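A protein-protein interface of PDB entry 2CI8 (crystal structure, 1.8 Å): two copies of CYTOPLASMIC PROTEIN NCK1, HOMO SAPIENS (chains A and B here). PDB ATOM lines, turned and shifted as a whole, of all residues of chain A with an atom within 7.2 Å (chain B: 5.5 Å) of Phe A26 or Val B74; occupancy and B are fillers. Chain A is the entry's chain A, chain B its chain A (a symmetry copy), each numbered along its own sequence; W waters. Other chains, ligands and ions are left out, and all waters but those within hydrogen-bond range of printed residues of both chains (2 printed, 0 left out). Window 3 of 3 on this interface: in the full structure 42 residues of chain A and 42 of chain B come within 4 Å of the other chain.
Water W1 lies within hydrogen-bond range of the side-chain carboxylate of Asp A25 (2.5 Å), a ring nitrogen (ND1) of His A22 (3.1 Å) and the side-chain amino group of Lys B95 (3.5 Å). Water W2 lies within hydrogen-bond range of the backbone carbonyl oxygen (O) of Trp A3 (2.6 Å), the backbone NH (N) of Ile A28 (2.8 Å), the backbone NH (N) of Tyr A5 (3.0 Å) and a ring nitrogen (ND1) of His B96 (3.3 Å).
No position is printed for both chains. Of the 19 pairs that touch across the chains among the printed residues, none has its exchanged pair printed and touching as well.
O of Ile A28 lies within hydrogen-bond range of N of Tyr A5 (2.8 Å). N of His A22 sits at hydrogen-bond distance from OD2 of Asp A25. O of Lys A43 is in hydrogen-bond range of N of Gly A24, at 2.8 Å. The backbone NH (N) of Lys A43 lies within hydrogen-bond range of the backbone carbonyl oxygen (O) of Asp A25 (3.0 Å). N of Ser A41 lies within hydrogen-bond range of O of Leu A27 (2.8 Å). The backbone NH (N) of Leu B93 sits at hydrogen-bond distance from the backbone carbonyl oxygen (O) of Tyr B77.
Hydrophobic or aromatic side chains of chain B that line the printed part of chain A: Met B70, Val B74, Leu B93, Val B94, His B96 and Leu B97.
Of the printed residues of chain B, Trp A3 touches Met B70 (3.4 Å), Glu B71 (3.4 Å) and His B96 (3.0 Å). Of the printed residues of chain B, Gly A21 touches Leu B97. Printed residues of chain B within 4 Å of Asp A25: Lys B95 (3.0 Å) and Leu B97 (3.9 Å). Printed residues of chain B within 4 Å of Phe A26: Val B74, Leu B93, Lys B95, His B96 and Leu B97. Of the printed residues of chain B, Ile A28 touches Met B70 (3.5 Å) and Val B74 (3.6 Å). Of the printed residues of chain A, Val B94 touches Gly A24 (2.8 Å). The nearest printed residue of chain B that does not touch Phe A26 is Val B94 (4.3 Å).
The backbone carbonyl oxygen (O) of Gly A24 is in hydrogen-bond range of the backbone NH (N) of Val B94 (2.8 Å). The backbone carbonyl oxygen (O) of Gly A24 is in hydrogen-bond range of the backbone NH (N) of Lys B95 (3.3 Å). OD1 of Asp A25 is in salt-bridge range of NZ of Lys B95 (3.0 Å). The backbone NH (N) of Phe A26 is in hydrogen-bond range of the backbone carbonyl oxygen (O) of Lys B95. The backbone NH (N) of Leu B97 lies within hydrogen-bond range of the backbone carbonyl oxygen (O) of Phe A26, 2.8 Å away.
Among the printed residues, pairs that only touch across the chains: Trp A3 with His B96 (3.0 Å), Phe A26 with His B96 (3.2 Å), Trp A3 with Met B70 (3.4 Å), Trp A3 with Glu B71 (3.4 Å), Gly A21 with Leu B97 (3.5 Å), Ile A28 with Met B70 (3.5 Å), Tyr A5 with Leu B97 (3.5 Å), Ile A28 with Val B74 (3.6 Å), Phe A26 with Val B74 (3.6 Å), Gly A24 with Leu B93 (3.8 Å), Leu A27 with Leu B97 (3.9 Å), Asp A25 with Leu B97 (3.9 Å), Leu A42 with Leu B93 (3.9 Å) and Phe A26 with Leu B93 (3.9 Å).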
ATOM      1  N   TRP A   3      23.316  -9.135   8.969  1.00  0.00           N
ATOM      2  CA  TRP A   3      24.373 -10.193   9.233  1.00  0.00           C
ATOM      3  C   TRP A   3      25.817  -9.693   9.285  1.00  0.00           C
ATOM      4  O   TRP A   3      26.715 -10.427   9.748  1.00  0.00           O
ATOM      5  CB  TRP A   3      24.379 -11.312   8.130  1.00  0.00           C
ATOM      6  CG  TRP A   3      24.612 -10.775   6.692  1.00  0.00           C
ATOM      7  CD1 TRP A   3      23.638 -10.477   5.785  1.00  0.00           C
ATOM      8  CD2 TRP A   3      25.866 -10.433   6.042  1.00  0.00           C
ATOM      9  NE1 TRP A   3      24.185  -9.981   4.623  1.00  0.00           N
ATOM     10  CE2 TRP A   3      25.545  -9.947   4.747  1.00  0.00           C
ATOM     11  CE3 TRP A   3      27.215 -10.489   6.421  1.00  0.00           C
ATOM     12  CZ2 TRP A   3      26.515  -9.540   3.833  1.00  0.00           C
ATOM     13  CZ3 TRP A   3      28.183 -10.095   5.501  1.00  0.00           C
ATOM     14  CH2 TRP A   3      27.824  -9.610   4.225  1.00  0.00           C
ATOM     15  N   TYR A   5      29.013  -7.280  10.555  1.00  0.00           N
ATOM     16  CA  TYR A   5      29.312  -6.565  11.777  1.00  0.00           C
ATOM     17  C   TYR A   5      29.965  -5.244  11.431  1.00  0.00           C
ATOM     18  O   TYR A   5      29.413  -4.185  11.722  1.00  0.00           O
ATOM     19  CB  TYR A   5      30.184  -7.418  12.674  1.00  0.00           C
ATOM     20  CG  TYR A   5      30.490  -6.866  13.995  1.00  0.00           C
ATOM     21  CD1 TYR A   5      31.579  -6.028  14.178  1.00  0.00           C
ATOM     22  CD2 TYR A   5      29.726  -7.227  15.112  1.00  0.00           C
ATOM     23  CE1 TYR A   5      31.896  -5.565  15.406  1.00  0.00           C
ATOM     24  CE2 TYR A   5      30.049  -6.760  16.372  1.00  0.00           C
ATOM     25  CZ  TYR A   5      31.127  -5.919  16.498  1.00  0.00           C
ATOM     26  OH  TYR A   5      31.450  -5.428  17.748  1.00  0.00           O
ATOM     27  N   LEU A  17      35.378 -10.028  20.738  1.00  0.00           N
ATOM     28  CA  LEU A  17      34.974 -11.351  21.271  1.00  0.00           C
ATOM     29  C   LEU A  17      35.517 -11.553  22.703  1.00  0.00           C
ATOM     30  O   LEU A  17      34.798 -12.098  23.557  1.00  0.00           O
ATOM     31  CB  LEU A  17      35.401 -12.458  20.348  1.00  0.00           C
ATOM     32  CG  LEU A  17      34.684 -12.534  18.980  1.00  0.00           C
ATOM     33  CD1 LEU A  17      35.538 -13.399  17.969  1.00  0.00           C
ATOM     34  CD2 LEU A  17      33.284 -13.029  19.217  1.00  0.00           C
ATOM     35  N   GLY A  21      32.083 -11.391  24.188  1.00  0.00           N
ATOM     36  CA  GLY A  21      31.652 -12.593  23.516  1.00  0.00           C
ATOM     37  C   GLY A  21      31.603 -13.773  24.450  1.00  0.00           C
ATOM     38  O   GLY A  21      32.280 -13.822  25.481  1.00  0.00           O
ATOM     39  N   HIS A  22      30.732 -14.707  24.086  1.00  0.00           N
ATOM     40  CA  HIS A  22      30.518 -15.918  24.805  1.00  0.00           C
ATOM     41  C   HIS A  22      30.522 -17.051  23.793  1.00  0.00           C
ATOM     42  O   HIS A  22      30.481 -16.793  22.581  1.00  0.00           O
ATOM     43  CB  HIS A  22      29.194 -15.800  25.534  1.00  0.00           C
ATOM     44  CG  HIS A  22      29.176 -14.698  26.547  1.00  0.00           C
ATOM     45  ND1 HIS A  22      28.594 -13.474  26.294  1.00  0.00           N
ATOM     46  CD2 HIS A  22      29.711 -14.614  27.783  1.00  0.00           C
ATOM     47  CE1 HIS A  22      28.747 -12.692  27.349  1.00  0.00           C
ATOM     48  NE2 HIS A  22      29.425 -13.360  28.266  1.00  0.00           N
ATOM     49  N   GLU A  23      30.886 -18.294  24.231  1.00  0.00           N
ATOM     50  CA  GLU A  23      30.726 -19.590  23.391  1.00  0.00           C
ATOM     51  C   GLU A  23      29.593 -19.471  22.344  1.00  0.00           C
ATOM     52  O   GLU A  23      28.410 -19.303  22.682  1.00  0.00           O
ATOM     53  CB  GLU A  23      30.381 -20.830  24.307  1.00  0.00           C
ATOM     54  CG  GLU A  23      30.307 -22.202  23.607  1.00  0.00           C
ATOM     55  CD  GLU A  23      31.647 -22.895  23.480  1.00  0.00           C
ATOM     56  OE1 GLU A  23      32.678 -22.246  23.670  1.00  0.00           O
ATOM     57  OE2 GLU A  23      31.667 -24.127  23.199  1.00  0.00           O
ATOM     58  N   GLY A  24      29.976 -19.575  21.083  1.00  0.00           N
ATOM     59  CA  GLY A  24      29.074 -19.571  19.941  1.00  0.00           C
ATOM     60  C   GLY A  24      28.758 -18.202  19.317  1.00  0.00           C
ATOM     61  O   GLY A  24      28.111 -18.115  18.266  1.00  0.00           O
ATOM     62  N   ASP A  25      29.195 -17.126  19.963  1.00  0.00           N
ATOM     63  CA  ASP A  25      28.981 -15.784  19.439  1.00  0.00           C
ATOM     64  C   ASP A  25      29.918 -15.603  18.226  1.00  0.00           C
ATOM     65  O   ASP A  25      31.040 -16.060  18.295  1.00  0.00           O
ATOM     66  CB  ASP A  25      29.366 -14.720  20.479  1.00  0.00           C
ATOM     67  CG  ASP A  25      28.273 -14.480  21.545  1.00  0.00           C
ATOM     68  OD1 ASP A  25      27.153 -14.935  21.332  1.00  0.00           O
ATOM     69  OD2 ASP A  25      28.558 -13.730  22.532  1.00  0.00           O
ATOM     70  N   PHE A  26      29.447 -14.899  17.203  1.00  0.00           N
ATOM     71  CA  PHE A  26      30.266 -14.676  15.998  1.00  0.00           C
ATOM     72  C   PHE A  26      29.987 -13.342  15.370  1.00  0.00           C
ATOM     73  O   PHE A  26      29.008 -12.658  15.681  1.00  0.00           O
ATOM     74  CB  PHE A  26      30.011 -15.781  14.965  1.00  0.00           C
ATOM     75  CG  PHE A  26      28.636 -15.745  14.380  1.00  0.00           C
ATOM     76  CD1 PHE A  26      27.572 -16.324  15.042  1.00  0.00           C
ATOM     77  CD2 PHE A  26      28.386 -15.120  13.198  1.00  0.00           C
ATOM     78  CE1 PHE A  26      26.291 -16.248  14.504  1.00  0.00           C
ATOM     79  CE2 PHE A  26      27.128 -15.054  12.678  1.00  0.00           C
ATOM     80  CZ  PHE A  26      26.069 -15.615  13.353  1.00  0.00           C
ATOM     81  N   LEU A  27      30.878 -12.952  14.472  1.00  0.00           N
ATOM     82  CA  LEU A  27      30.697 -11.758  13.716  1.00  0.00           C
ATOM     83  C   LEU A  27      31.265 -12.006  12.338  1.00  0.00           C
ATOM     84  O   LEU A  27      32.122 -12.898  12.168  1.00  0.00           O
ATOM     85  CB  LEU A  27      31.328 -10.563  14.436  1.00  0.00           C
ATOM     86  CG  LEU A  27      32.844 -10.549  14.695  1.00  0.00           C
ATOM     87  CD1 LEU A  27      33.569  -9.951  13.511  1.00  0.00           C
ATOM     88  CD2 LEU A  27      33.168  -9.795  15.933  1.00  0.00           C
ATOM     89  N   ILE A  28      30.730 -11.289  11.359  1.00  0.00           N
ATOM     90  CA  ILE A  28      31.166 -11.388   9.960  1.00  0.00           C
ATOM     91  C   ILE A  28      31.734 -10.027   9.577  1.00  0.00           C
ATOM     92  O   ILE A  28      31.058  -9.025   9.726  1.00  0.00           O
ATOM     93  CB  ILE A  28      30.037 -11.825   9.018  1.00  0.00           C
ATOM     94  CG1 ILE A  28      29.454 -13.210   9.476  1.00  0.00           C
ATOM     95  CG2 ILE A  28      30.562 -11.925   7.606  1.00  0.00           C
ATOM     96  CD1 ILE A  28      28.312 -13.702   8.616  1.00  0.00           C
ATOM     97  N   VAL A  40      34.392 -15.059   9.033  1.00  0.00           N
ATOM     98  CA  VAL A  40      33.476 -15.320  10.152  1.00  0.00           C
ATOM     99  C   VAL A  40      34.372 -15.539  11.390  1.00  0.00           C
ATOM    100  O   VAL A  40      35.221 -16.401  11.372  1.00  0.00           O
ATOM    101  CB  VAL A  40      32.666 -16.606   9.904  1.00  0.00           C
ATOM    102  CG1 VAL A  40      31.849 -16.965  11.198  1.00  0.00           C
ATOM    103  CG2 VAL A  40      31.751 -16.427   8.700  1.00  0.00           C
ATOM    104  N   SER A  41      34.230 -14.729  12.437  1.00  0.00           N
ATOM    105  CA  SER A  41      35.090 -14.798  13.625  1.00  0.00           C
ATOM    106  C   SER A  41      34.173 -15.303  14.743  1.00  0.00           C
ATOM    107  O   SER A  41      33.129 -14.721  14.976  1.00  0.00           O
ATOM    108  CB  SER A  41      35.697 -13.448  13.983  1.00  0.00           C
ATOM    109  OG  SER A  41      36.580 -13.004  12.933  1.00  0.00           O
ATOM    110  N   LEU A  42      34.587 -16.415  15.351  1.00  0.00           N
ATOM    111  CA  LEU A  42      33.770 -17.195  16.274  1.00  0.00           C
ATOM    112  C   LEU A  42      34.514 -17.409  17.554  1.00  0.00           C
ATOM    113  O   LEU A  42      35.679 -17.743  17.542  1.00  0.00           O
ATOM    114  CB  LEU A  42      33.458 -18.577  15.623  1.00  0.00           C
ATOM    115  CG  LEU A  42      32.721 -19.633  16.484  1.00  0.00           C
ATOM    116  CD1 LEU A  42      31.354 -19.155  16.796  1.00  0.00           C
ATOM    117  CD2 LEU A  42      32.688 -21.039  15.829  1.00  0.00           C
ATOM    118  N   LYS A  43      33.794 -17.271  18.693  1.00  0.00           N
ATOM    119  CA  LYS A  43      34.341 -17.617  19.999  1.00  0.00           C
ATOM    120  C   LYS A  43      33.840 -19.060  20.318  1.00  0.00           C
ATOM    121  O   LYS A  43      32.677 -19.295  20.261  1.00  0.00           O
ATOM    122  CB  LYS A  43      33.834 -16.646  21.057  1.00  0.00           C
ATOM    123  CG  LYS A  43      34.479 -16.912  22.429  1.00  0.00           C
ATOM    124  CD  LYS A  43      34.181 -15.808  23.392  1.00  0.00           C
ATOM    125  CE  LYS A  43      34.991 -15.940  24.693  1.00  0.00           C
ATOM    126  NZ  LYS A  43      35.205 -14.618  25.311  1.00  0.00           N
ATOM    127  N   THR B  69      23.355 -16.490  -0.286  1.00  0.00           N
ATOM    128  CA  THR B  69      23.327 -15.344   0.603  1.00  0.00           C
ATOM    129  C   THR B  69      24.102 -15.660   1.882  1.00  0.00           C
ATOM    130  O   THR B  69      24.212 -16.826   2.304  1.00  0.00           O
ATOM    131  CB  THR B  69      21.896 -14.988   1.016  1.00  0.00           C
ATOM    132  OG1 THR B  69      21.363 -16.030   1.822  1.00  0.00           O
ATOM    133  CG2 THR B  69      20.994 -14.764  -0.180  1.00  0.00           C
ATOM    134  N   MET B  70      24.562 -14.610   2.553  1.00  0.00           N
ATOM    135  CA  MET B  70      25.222 -14.779   3.842  1.00  0.00           C
ATOM    136  C   MET B  70      24.244 -15.278   4.923  1.00  0.00           C
ATOM    137  O   MET B  70      24.645 -16.049   5.803  1.00  0.00           O
ATOM    138  CB  MET B  70      25.921 -13.478   4.272  1.00  0.00           C
ATOM    139  CG  MET B  70      26.924 -13.671   5.413  1.00  0.00           C
ATOM    140  SD  MET B  70      28.384 -14.569   4.955  1.00  0.00           S
ATOM    141  CE  MET B  70      29.372 -13.350   4.089  1.00  0.00           C
ATOM    142  N   GLU B  71      22.959 -14.881   4.852  1.00  0.00           N
ATOM    143  CA  GLU B  71      21.983 -15.368   5.823  1.00  0.00           C
ATOM    144  C   GLU B  71      21.875 -16.875   5.763  1.00  0.00           C
ATOM    145  O   GLU B  71      21.882 -17.535   6.803  1.00  0.00           O
ATOM    146  CB  GLU B  71      20.604 -14.720   5.666  1.00  0.00           C
ATOM    147  CG  GLU B  71      20.553 -13.225   6.027  1.00  0.00           C
ATOM    148  CD  GLU B  71      20.847 -12.275   4.852  1.00  0.00           C
ATOM    149  OE1 GLU B  71      21.495 -12.669   3.847  1.00  0.00           O
ATOM    150  OE2 GLU B  71      20.432 -11.089   4.964  1.00  0.00           O
ATOM    151  N   GLU B  72      21.823 -17.435   4.549  1.00  0.00           N
ATOM    152  CA  GLU B  72      21.804 -18.912   4.380  1.00  0.00           C
ATOM    153  C   GLU B  72      23.022 -19.588   4.956  1.00  0.00           C
ATOM    154  O   GLU B  72      22.918 -20.636   5.622  1.00  0.00           O
ATOM    155  CB  GLU B  72      21.715 -19.305   2.906  1.00  0.00           C
ATOM    156  CG  GLU B  72      20.349 -19.189   2.267  1.00  0.00           C
ATOM    157  CD  GLU B  72      20.266 -19.973   0.946  1.00  0.00           C
ATOM    158  OE1 GLU B  72      19.169 -20.032   0.355  1.00  0.00           O
ATOM    159  OE2 GLU B  72      21.298 -20.541   0.506  1.00  0.00           O
ATOM    160  N   LEU B  73      24.186 -19.004   4.682  1.00  0.00           N
ATOM    161  CA  LEU B  73      25.448 -19.483   5.243  1.00  0.00           C
ATOM    162  C   LEU B  73      25.340 -19.559   6.769  1.00  0.00           C
ATOM    163  O   LEU B  73      25.497 -20.629   7.380  1.00  0.00           O
ATOM    164  CB  LEU B  73      26.595 -18.559   4.767  1.00  0.00           C
ATOM    165  CG  LEU B  73      28.045 -18.930   5.108  1.00  0.00           C
ATOM    166  CD1 LEU B  73      29.044 -18.318   4.089  1.00  0.00           C
ATOM    167  CD2 LEU B  73      28.386 -18.458   6.543  1.00  0.00           C
ATOM    168  N   VAL B  74      24.961 -18.438   7.382  1.00  0.00           N
ATOM    169  CA  VAL B  74      24.834 -18.376   8.844  1.00  0.00           C
ATOM    170  C   VAL B  74      23.899 -19.465   9.434  1.00  0.00           C
ATOM    171  O   VAL B  74      24.308 -20.245  10.307  1.00  0.00           O
ATOM    172  CB  VAL B  74      24.414 -16.960   9.294  1.00  0.00           C
ATOM    173  CG1 VAL B  74      23.937 -16.976  10.762  1.00  0.00           C
ATOM    174  CG2 VAL B  74      25.583 -15.977   9.100  1.00  0.00           C
ATOM    175  N   GLU B  75      22.681 -19.555   8.913  1.00  0.00           N
ATOM    176  CA  GLU B  75      21.731 -20.595   9.379  1.00  0.00           C
ATOM    177  C   GLU B  75      22.260 -22.009   9.232  1.00  0.00           C
ATOM    178  O   GLU B  75      22.124 -22.833  10.129  1.00  0.00           O
ATOM    179  CB  GLU B  75      20.388 -20.465   8.665  1.00  0.00           C
ATOM    180  CG  GLU B  75      19.622 -19.190   9.025  1.00  0.00           C
ATOM    181  CD  GLU B  75      19.369 -19.065  10.536  1.00  0.00           C
ATOM    182  OE1 GLU B  75      19.049 -20.104  11.174  1.00  0.00           O
ATOM    183  OE2 GLU B  75      19.518 -17.937  11.073  1.00  0.00           O
ATOM    184  N   HIS B  76      22.876 -22.301   8.097  1.00  0.00           N
ATOM    185  CA  HIS B  76      23.444 -23.597   7.878  1.00  0.00           C
ATOM    186  C   HIS B  76      24.434 -24.008   8.944  1.00  0.00           C
ATOM    187  O   HIS B  76      24.426 -25.167   9.404  1.00  0.00           O
ATOM    188  CB  HIS B  76      24.105 -23.629   6.504  1.00  0.00           C
ATOM    189  CG  HIS B  76      24.694 -24.944   6.166  1.00  0.00           C
ATOM    190  ND1 HIS B  76      23.974 -25.934   5.549  1.00  0.00           N
ATOM    191  CD2 HIS B  76      25.925 -25.450   6.389  1.00  0.00           C
ATOM    192  CE1 HIS B  76      24.743 -26.987   5.382  1.00  0.00           C
ATOM    193  NE2 HIS B  76      25.933 -26.719   5.884  1.00  0.00           N
ATOM    194  N   TYR B  77      25.291 -23.058   9.353  1.00  0.00           N
ATOM    195  CA  TYR B  77      26.292 -23.337  10.340  1.00  0.00           C
ATOM    196  C   TYR B  77      25.876 -23.232  11.813  1.00  0.00           C
ATOM    197  O   TYR B  77      26.697 -23.465  12.706  1.00  0.00           O
ATOM    198  CB  TYR B  77      27.557 -22.588   9.999  1.00  0.00           C
ATOM    199  CG  TYR B  77      28.176 -23.168   8.757  1.00  0.00           C
ATOM    200  CD1 TYR B  77      28.751 -24.431   8.789  1.00  0.00           C
ATOM    201  CD2 TYR B  77      28.204 -22.473   7.563  1.00  0.00           C
ATOM    202  CE1 TYR B  77      29.345 -25.006   7.639  1.00  0.00           C
ATOM    203  CE2 TYR B  77      28.818 -23.029   6.418  1.00  0.00           C
ATOM    204  CZ  TYR B  77      29.374 -24.299   6.475  1.00  0.00           C
ATOM    205  OH  TYR B  77      29.966 -24.875   5.354  1.00  0.00           O
ATOM    206  N   LYS B  78      24.602 -22.936  12.030  1.00  0.00           N
ATOM    207  CA  LYS B  78      23.952 -23.060  13.336  1.00  0.00           C
ATOM    208  C   LYS B  78      23.448 -24.502  13.550  1.00  0.00           C
ATOM    209  O   LYS B  78      23.354 -24.959  14.698  1.00  0.00           O
ATOM    210  CB  LYS B  78      22.789 -22.083  13.455  1.00  0.00           C
ATOM    211  CG  LYS B  78      23.207 -20.633  13.620  1.00  0.00           C
ATOM    212  CD  LYS B  78      22.012 -19.692  13.642  1.00  0.00           C
ATOM    213  CE  LYS B  78      22.453 -18.243  13.868  1.00  0.00           C
ATOM    214  NZ  LYS B  78      21.336 -17.294  13.829  1.00  0.00           N
ATOM    215  N   LEU B  93      27.977 -22.128  15.022  1.00  0.00           N
ATOM    216  CA  LEU B  93      27.651 -20.737  15.219  1.00  0.00           C
ATOM    217  C   LEU B  93      26.414 -20.791  16.147  1.00  0.00           C
ATOM    218  O   LEU B  93      25.621 -21.684  16.007  1.00  0.00           O
ATOM    219  CB  LEU B  93      27.241 -20.073  13.909  1.00  0.00           C
ATOM    220  CG  LEU B  93      28.320 -19.994  12.779  1.00  0.00           C
ATOM    221  CD1 LEU B  93      27.895 -19.114  11.625  1.00  0.00           C
ATOM    222  CD2 LEU B  93      29.606 -19.551  13.316  1.00  0.00           C
ATOM    223  N   VAL B  94      26.266 -19.840  17.048  1.00  0.00           N
ATOM    224  CA  VAL B  94      25.063 -19.794  17.951  1.00  0.00           C
ATOM    225  C   VAL B  94      24.295 -18.472  17.709  1.00  0.00           C
ATOM    226  O   VAL B  94      23.123 -18.501  17.271  1.00  0.00           O
ATOM    227  CB  VAL B  94      25.453 -20.106  19.422  1.00  0.00           C
ATOM    228  CG1 VAL B  94      24.253 -19.966  20.363  1.00  0.00           C
ATOM    229  CG2 VAL B  94      26.046 -21.527  19.521  1.00  0.00           C
ATOM    230  N   LYS B  95      24.927 -17.302  17.936  1.00  0.00           N
ATOM    231  CA  LYS B  95      24.289 -16.013  17.572  1.00  0.00           C
ATOM    232  C   LYS B  95      25.295 -14.894  17.327  1.00  0.00           C
ATOM    233  O   LYS B  95      26.431 -14.991  17.740  1.00  0.00           O
ATOM    234  CB  LYS B  95      23.297 -15.558  18.657  1.00  0.00           C
ATOM    235  CG  LYS B  95      23.927 -15.393  20.018  1.00  0.00           C
ATOM    236  CD  LYS B  95      22.949 -14.733  20.994  1.00  0.00           C
ATOM    237  CE  LYS B  95      23.633 -14.366  22.273  1.00  0.00           C
ATOM    238  NZ  LYS B  95      24.702 -13.333  22.079  1.00  0.00           N
ATOM    239  N   HIS B  96      24.824 -13.831  16.707  1.00  0.00           N
ATOM    240  CA  HIS B  96      25.647 -12.658  16.378  1.00  0.00           C
ATOM    241  C   HIS B  96      26.146 -11.987  17.668  1.00  0.00           C
ATOM    242  O   HIS B  96      25.423 -11.964  18.674  1.00  0.00           O
ATOM    243  CB  HIS B  96      24.876 -11.654  15.486  1.00  0.00           C
ATOM    244  CG  HIS B  96      24.936 -12.024  14.025  1.00  0.00           C
ATOM    245  ND1 HIS B  96      26.075 -11.883  13.259  1.00  0.00           N
ATOM    246  CD2 HIS B  96      23.977 -12.491  13.178  1.00  0.00           C
ATOM    247  CE1 HIS B  96      25.816 -12.241  12.012  1.00  0.00           C
ATOM    248  NE2 HIS B  96      24.552 -12.628  11.939  1.00  0.00           N
ATOM    249  N   LEU B  97      27.404 -11.527  17.652  1.00  0.00           N
ATOM    250  CA  LEU B  97      27.945 -10.690  18.729  1.00  0.00           C
ATOM    251  C   LEU B  97      27.248  -9.332  18.597  1.00  0.00           C
ATOM    252  O   LEU B  97      27.321  -8.690  17.547  1.00  0.00           O
ATOM    253  CB  LEU B  97      29.451 -10.461  18.575  1.00  0.00           C
ATOM    254  CG  LEU B  97      30.169  -9.734  19.755  1.00  0.00           C
ATOM    255  CD1 LEU B  97      30.316 -10.656  20.947  1.00  0.00           C
ATOM    256  CD2 LEU B  97      31.469  -9.229  19.369  1.00  0.00           C
HETATM  257  O   HOH W   1      27.401 -12.008  23.842  1.00  0.00           O
HETATM  258  O   HOH W   2      28.281  -9.919  11.734  1.00  0.00           O
